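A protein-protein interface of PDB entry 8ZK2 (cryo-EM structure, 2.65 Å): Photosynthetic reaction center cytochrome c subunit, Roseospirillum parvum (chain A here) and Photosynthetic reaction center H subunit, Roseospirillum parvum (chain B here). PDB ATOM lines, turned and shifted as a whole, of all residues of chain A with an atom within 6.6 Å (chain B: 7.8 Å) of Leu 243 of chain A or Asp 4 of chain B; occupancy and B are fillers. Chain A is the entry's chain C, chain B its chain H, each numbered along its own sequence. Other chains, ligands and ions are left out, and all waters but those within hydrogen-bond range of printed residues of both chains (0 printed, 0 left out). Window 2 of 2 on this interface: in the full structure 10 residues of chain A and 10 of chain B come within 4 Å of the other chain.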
ATOM      1  N   PRO A 239       5.316   2.826 -11.702  1.00  0.00           N
ATOM      2  CA  PRO A 239       5.110   2.315 -10.345  1.00  0.00           C
ATOM      3  C   PRO A 239       4.207   3.222  -9.528  1.00  0.00           C
ATOM      4  O   PRO A 239       4.127   4.431  -9.755  1.00  0.00           O
ATOM      5  CB  PRO A 239       6.526   2.281  -9.767  1.00  0.00           C
ATOM      6  CG  PRO A 239       7.258   3.304 -10.557  1.00  0.00           C
ATOM      7  CD  PRO A 239       6.725   3.171 -11.942  1.00  0.00           C
ATOM      8  N   ASN A 241       4.745   3.657  -6.363  1.00  0.00           N
ATOM      9  CA  ASN A 241       5.580   4.161  -5.286  1.00  0.00           C
ATOM     10  C   ASN A 241       6.783   4.883  -5.876  1.00  0.00           C
ATOM     11  O   ASN A 241       7.231   4.580  -6.982  1.00  0.00           O
ATOM     12  CB  ASN A 241       6.053   3.036  -4.360  1.00  0.00           C
ATOM     13  CG  ASN A 241       6.589   3.556  -3.048  1.00  0.00           C
ATOM     14  OD1 ASN A 241       7.592   3.066  -2.539  1.00  0.00           O
ATOM     15  ND2 ASN A 241       5.919   4.556  -2.492  1.00  0.00           N
ATOM     16  N   ASP A 242       7.306   5.847  -5.117  1.00  0.00           N
ATOM     17  CA  ASP A 242       8.454   6.617  -5.584  1.00  0.00           C
ATOM     18  C   ASP A 242       9.748   5.820  -5.531  1.00  0.00           C
ATOM     19  O   ASP A 242      10.660   6.074  -6.324  1.00  0.00           O
ATOM     20  CB  ASP A 242       8.598   7.899  -4.764  1.00  0.00           C
ATOM     21  CG  ASP A 242       8.777   7.632  -3.286  1.00  0.00           C
ATOM     22  OD1 ASP A 242       7.925   6.934  -2.697  1.00  0.00           O
ATOM     23  OD2 ASP A 242       9.764   8.129  -2.708  1.00  0.00           O
ATOM     24  N   LEU A 243       9.849   4.864  -4.620  1.00  0.00           N
ATOM     25  CA  LEU A 243      11.064   4.085  -4.489  1.00  0.00           C
ATOM     26  C   LEU A 243      10.821   2.646  -4.922  1.00  0.00           C
ATOM     27  O   LEU A 243       9.698   2.145  -4.800  1.00  0.00           O
ATOM     28  CB  LEU A 243      11.570   4.105  -3.043  1.00  0.00           C
ATOM     29  CG  LEU A 243      11.944   5.480  -2.488  1.00  0.00           C
ATOM     30  CD1 LEU A 243      12.766   5.335  -1.233  1.00  0.00           C
ATOM     31  CD2 LEU A 243      12.690   6.309  -3.518  1.00  0.00           C
ATOM     32  N   PRO A 244      11.838   1.966  -5.447  1.00  0.00           N
ATOM     33  CA  PRO A 244      11.654   0.571  -5.858  1.00  0.00           C
ATOM     34  C   PRO A 244      11.329  -0.323  -4.672  1.00  0.00           C
ATOM     35  O   PRO A 244      11.778  -0.087  -3.549  1.00  0.00           O
ATOM     36  CB  PRO A 244      13.006   0.208  -6.480  1.00  0.00           C
ATOM     37  CG  PRO A 244      13.592   1.511  -6.882  1.00  0.00           C
ATOM     38  CD  PRO A 244      13.173   2.463  -5.812  1.00  0.00           C
ATOM     39  N   MET A 245      10.529  -1.351  -4.931  1.00  0.00           N
ATOM     40  CA  MET A 245      10.231  -2.384  -3.956  1.00  0.00           C
ATOM     41  C   MET A 245      11.159  -3.577  -4.161  1.00  0.00           C
ATOM     42  O   MET A 245      11.909  -3.660  -5.136  1.00  0.00           O
ATOM     43  CB  MET A 245       8.767  -2.810  -4.051  1.00  0.00           C
ATOM     44  CG  MET A 245       7.760  -1.740  -3.685  1.00  0.00           C
ATOM     45  SD  MET A 245       7.909  -1.256  -1.960  1.00  0.00           S
ATOM     46  CE  MET A 245       6.787   0.131  -1.914  1.00  0.00           C
ATOM     47  N   MET B   1      11.194  -1.393   0.524  1.00  0.00           N
ATOM     48  CA  MET B   1      11.865  -0.248  -0.078  1.00  0.00           C
ATOM     49  C   MET B   1      13.287  -0.634  -0.460  1.00  0.00           C
ATOM     50  O   MET B   1      13.819  -1.620   0.044  1.00  0.00           O
ATOM     51  CB  MET B   1      11.883   0.936   0.885  1.00  0.00           C
ATOM     52  CG  MET B   1      10.516   1.500   1.221  1.00  0.00           C
ATOM     53  SD  MET B   1       9.640   2.205  -0.179  1.00  0.00           S
ATOM     54  CE  MET B   1       8.046   2.517   0.573  1.00  0.00           C
ATOM     55  N   ILE B   2      13.909   0.138  -1.344  1.00  0.00           N
ATOM     56  CA  ILE B   2      15.276  -0.111  -1.779  1.00  0.00           C
ATOM     57  C   ILE B   2      16.188   1.071  -1.471  1.00  0.00           C
ATOM     58  O   ILE B   2      17.157   0.936  -0.725  1.00  0.00           O
ATOM     59  CB  ILE B   2      15.327  -0.482  -3.280  1.00  0.00           C
ATOM     60  CG1 ILE B   2      14.962  -1.955  -3.466  1.00  0.00           C
ATOM     61  CG2 ILE B   2      16.704  -0.223  -3.858  1.00  0.00           C
ATOM     62  CD1 ILE B   2      14.947  -2.406  -4.898  1.00  0.00           C
ATOM     63  N   GLY B   3      15.881   2.244  -2.016  1.00  0.00           N
ATOM     64  CA  GLY B   3      16.794   3.362  -1.888  1.00  0.00           C
ATOM     65  C   GLY B   3      16.441   4.354  -0.801  1.00  0.00           C
ATOM     66  O   GLY B   3      16.566   5.562  -1.006  1.00  0.00           O
ATOM     67  N   ASP B   4      16.013   3.869   0.359  1.00  0.00           N
ATOM     68  CA  ASP B   4      15.524   4.727   1.428  1.00  0.00           C
ATOM     69  C   ASP B   4      16.457   4.690   2.631  1.00  0.00           C
ATOM     70  O   ASP B   4      17.017   3.642   2.968  1.00  0.00           O
ATOM     71  CB  ASP B   4      14.112   4.317   1.855  1.00  0.00           C
ATOM     72  CG  ASP B   4      14.086   3.007   2.609  1.00  0.00           C
ATOM     73  OD1 ASP B   4      14.655   2.018   2.106  1.00  0.00           O
ATOM     74  OD2 ASP B   4      13.488   2.962   3.703  1.00  0.00           O
ATOM     75  N   PHE B   5      16.629   5.851   3.267  1.00  0.00           N
ATOM     76  CA  PHE B   5      17.256   5.947   4.575  1.00  0.00           C
ATOM     77  C   PHE B   5      16.246   6.109   5.696  1.00  0.00           C
ATOM     78  O   PHE B   5      16.548   5.748   6.837  1.00  0.00           O
ATOM     79  CB  PHE B   5      18.231   7.132   4.621  1.00  0.00           C
ATOM     80  CG  PHE B   5      19.338   7.047   3.616  1.00  0.00           C
ATOM     81  CD1 PHE B   5      20.110   5.908   3.513  1.00  0.00           C
ATOM     82  CD2 PHE B   5      19.608   8.108   2.774  1.00  0.00           C
ATOM     83  CE1 PHE B   5      21.127   5.828   2.588  1.00  0.00           C
ATOM     84  CE2 PHE B   5      20.625   8.028   1.849  1.00  0.00           C
ATOM     85  CZ  PHE B   5      21.386   6.889   1.758  1.00  0.00           C
ATOM     86  N   SER B   6      15.066   6.633   5.395  1.00  0.00           N
ATOM     87  CA  SER B   6      14.006   6.853   6.366  1.00  0.00           C
ATOM     88  C   SER B   6      12.691   6.903   5.600  1.00  0.00           C
ATOM     89  O   SER B   6      12.632   6.565   4.413  1.00  0.00           O
ATOM     90  CB  SER B   6      14.260   8.132   7.168  1.00  0.00           C
ATOM     91  OG  SER B   6      13.228   8.352   8.112  1.00  0.00           O
ATOM     92  N   SER B   7      11.628   7.327   6.277  1.00  0.00           N
ATOM     93  CA  SER B   7      10.346   7.530   5.619  1.00  0.00           C
ATOM     94  C   SER B   7      10.327   8.772   4.740  1.00  0.00           C
ATOM     95  O   SER B   7       9.423   8.910   3.911  1.00  0.00           O
ATOM     96  CB  SER B   7       9.227   7.622   6.660  1.00  0.00           C
ATOM     97  OG  SER B   7       9.375   8.778   7.464  1.00  0.00           O
ATOM     98  N   TYR B   8      11.292   9.674   4.905  1.00  0.00           N
ATOM     99  CA  TYR B   8      11.407  10.868   4.081  1.00  0.00           C
ATOM    100  C   TYR B   8      12.691  10.891   3.271  1.00  0.00           C
ATOM    101  O   TYR B   8      12.650  11.119   2.057  1.00  0.00           O
ATOM    102  CB  TYR B   8      11.328  12.129   4.957  1.00  0.00           C
ATOM    103  CG  TYR B   8      11.287  13.415   4.164  1.00  0.00           C
ATOM    104  CD1 TYR B   8      10.095  13.895   3.644  1.00  0.00           C
ATOM    105  CD2 TYR B   8      12.445  14.141   3.923  1.00  0.00           C
ATOM    106  CE1 TYR B   8      10.055  15.065   2.917  1.00  0.00           C
ATOM    107  CE2 TYR B   8      12.413  15.310   3.194  1.00  0.00           C
ATOM    108  CZ  TYR B   8      11.217  15.769   2.695  1.00  0.00           C
ATOM    109  OH  TYR B   8      11.185  16.936   1.970  1.00  0.00           O
ATOM    110  N   MET B   9      13.834  10.665   3.910  1.00  0.00           N
ATOM    111  CA  MET B   9      15.116  10.729   3.230  1.00  0.00           C
ATOM    112  C   MET B   9      15.337   9.488   2.375  1.00  0.00           C
ATOM    113  O   MET B   9      14.792   8.415   2.645  1.00  0.00           O
ATOM    114  CB  MET B   9      16.249  10.874   4.245  1.00  0.00           C
ATOM    115  CG  MET B   9      16.401  12.280   4.801  1.00  0.00           C
ATOM    116  SD  MET B   9      17.811  12.442   5.907  1.00  0.00           S
ATOM    117  CE  MET B   9      17.838  10.816   6.647  1.00  0.00           C
ATOM    118  N   ASP B  10      16.146   9.645   1.330  1.00  0.00           N
ATOM    119  CA  ASP B  10      16.445   8.558   0.411  1.00  0.00           C
ATOM    120  C   ASP B  10      17.775   8.838  -0.279  1.00  0.00           C
ATOM    121  O   ASP B  10      18.383   9.898  -0.100  1.00  0.00           O
ATOM    122  CB  ASP B  10      15.305   8.363  -0.593  1.00  0.00           C
ATOM    123  CG  ASP B  10      14.943   9.633  -1.319  1.00  0.00           C
ATOM    124  OD1 ASP B  10      15.504  10.692  -0.986  1.00  0.00           O
ATOM    125  OD2 ASP B  10      14.084   9.576  -2.215  1.00  0.00           O
ATOM    126  N   VAL B  11      18.228   7.870  -1.077  1.00  0.00           N
ATOM    127  CA  VAL B  11      19.557   7.941  -1.674  1.00  0.00           C
ATOM    128  C   VAL B  11      19.662   9.067  -2.695  1.00  0.00           C
ATOM    129  O   VAL B  11      20.681   9.764  -2.748  1.00  0.00           O
ATOM    130  CB  VAL B  11      19.925   6.582  -2.295  1.00  0.00           C
ATOM    131  CG1 VAL B  11      21.278   6.652  -2.981  1.00  0.00           C
ATOM    132  CG2 VAL B  11      19.923   5.499  -1.232  1.00  0.00           C
ATOM    133  N   ALA B  12      18.632   9.266  -3.521  1.00  0.00           N
ATOM    134  CA  ALA B  12      18.689  10.307  -4.542  1.00  0.00           C
ATOM    135  C   ALA B  12      18.804  11.697  -3.929  1.00  0.00           C
ATOM    136  O   ALA B  12      19.541  12.541  -4.443  1.00  0.00           O
ATOM    137  CB  ALA B  12      17.461  10.229  -5.445  1.00  0.00           C
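The side-chain sulfur of Met 1 of chain B sits close to the side-chain amide oxygen of Asn 241 of chain A, at 3.2 Å.
O of Pro 244 of chain A is in hydrogen-bond range of N of Ile 2 of chain B (3.1 Å).
ND2 of Asn 241 of chain A is in hydrogen-bond range of OD1 of Asp 242 of chain A (3.1 Å).
The side-chain amide oxygen of Asn 241 of chain A sits close to the backbone carbonyl oxygen of Leu 243 of chain A (3.2 Å).
The backbone carbonyl oxygen (O) of Gly 3 of chain B sits at hydrogen-bond distance from the backbone NH (N) of Val 11 of chain B, 2.8 Å away.
Among the printed residues, pairs that only touch across the chains: Met 245 of chain A with Ile 2 of chain B, Pro 244 of chain A with Met 1 of chain B, Leu 243 of chain A with Asp 4 of chain B, Met 245 of chain A with Met 1 of chain B, Leu 243 of chain A with Asp 10 of chain B, Leu 243 of chain A with Gly 3 of chain B and Leu 243 of chain A with Met 1 of chain B.
Of the printed residues of chain B, Asn 241 of chain A touches Met 1 (3.2 Å).
No residue of chain B comes within 4 Å of Asp 242 of chain A.
Leu 243 of chain A touches just these residues of chain B: Met 1, Gly 3, Asp 4 and Asp 10.
Pro 244 of chain A touches two residues of chain B.
Of the printed residues of chain B, Met 245 of chain A touches Met 1 and Ile 2.
Of the printed residues of chain A, Met 1 of chain B touches Asn 241, Leu 243, Pro 244 and Met 245.
Printed residues of chain A within 4 Å of Gly 3 of chain B: Leu 243 (3.8 Å).
Asp 4 of chain B touches just one residue of chain A: Leu 243 (3.5 Å).
Met 9 of chain B touches none of the printed residues of chain A.
Of the printed residues of chain A, Asp 10 of chain B touches Leu 243.
The nearest printed residue of chain A that does not touch Asp 4 of chain B is Pro 244 of chain A (6.7 Å).
Of the 12 printed residues of chain B, 5 touch a printed residue of chain A.
Hydrophobic or aromatic side chains of chain B that line the printed part of chain A: Met 1 and Ile 2.
Along chain B the printed residues that touch a printed residue of chain A span positions 1 to 10.
Of the 6 printed residues of chain A, 4 touch a printed residue of chain B.
Printed residues of chain A that touch a printed residue of chain B: Asn 241, Leu 243, Pro 244 and Met 245.
Hydrophobic or aromatic side chains of chain A that line the printed part of chain B: Leu 243, Pro 244 and Met 245.
Along chain A the printed residues that touch a printed residue of chain B span positions 241 to 245.
Among the printed residues, 9 pairs touch across the chains.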
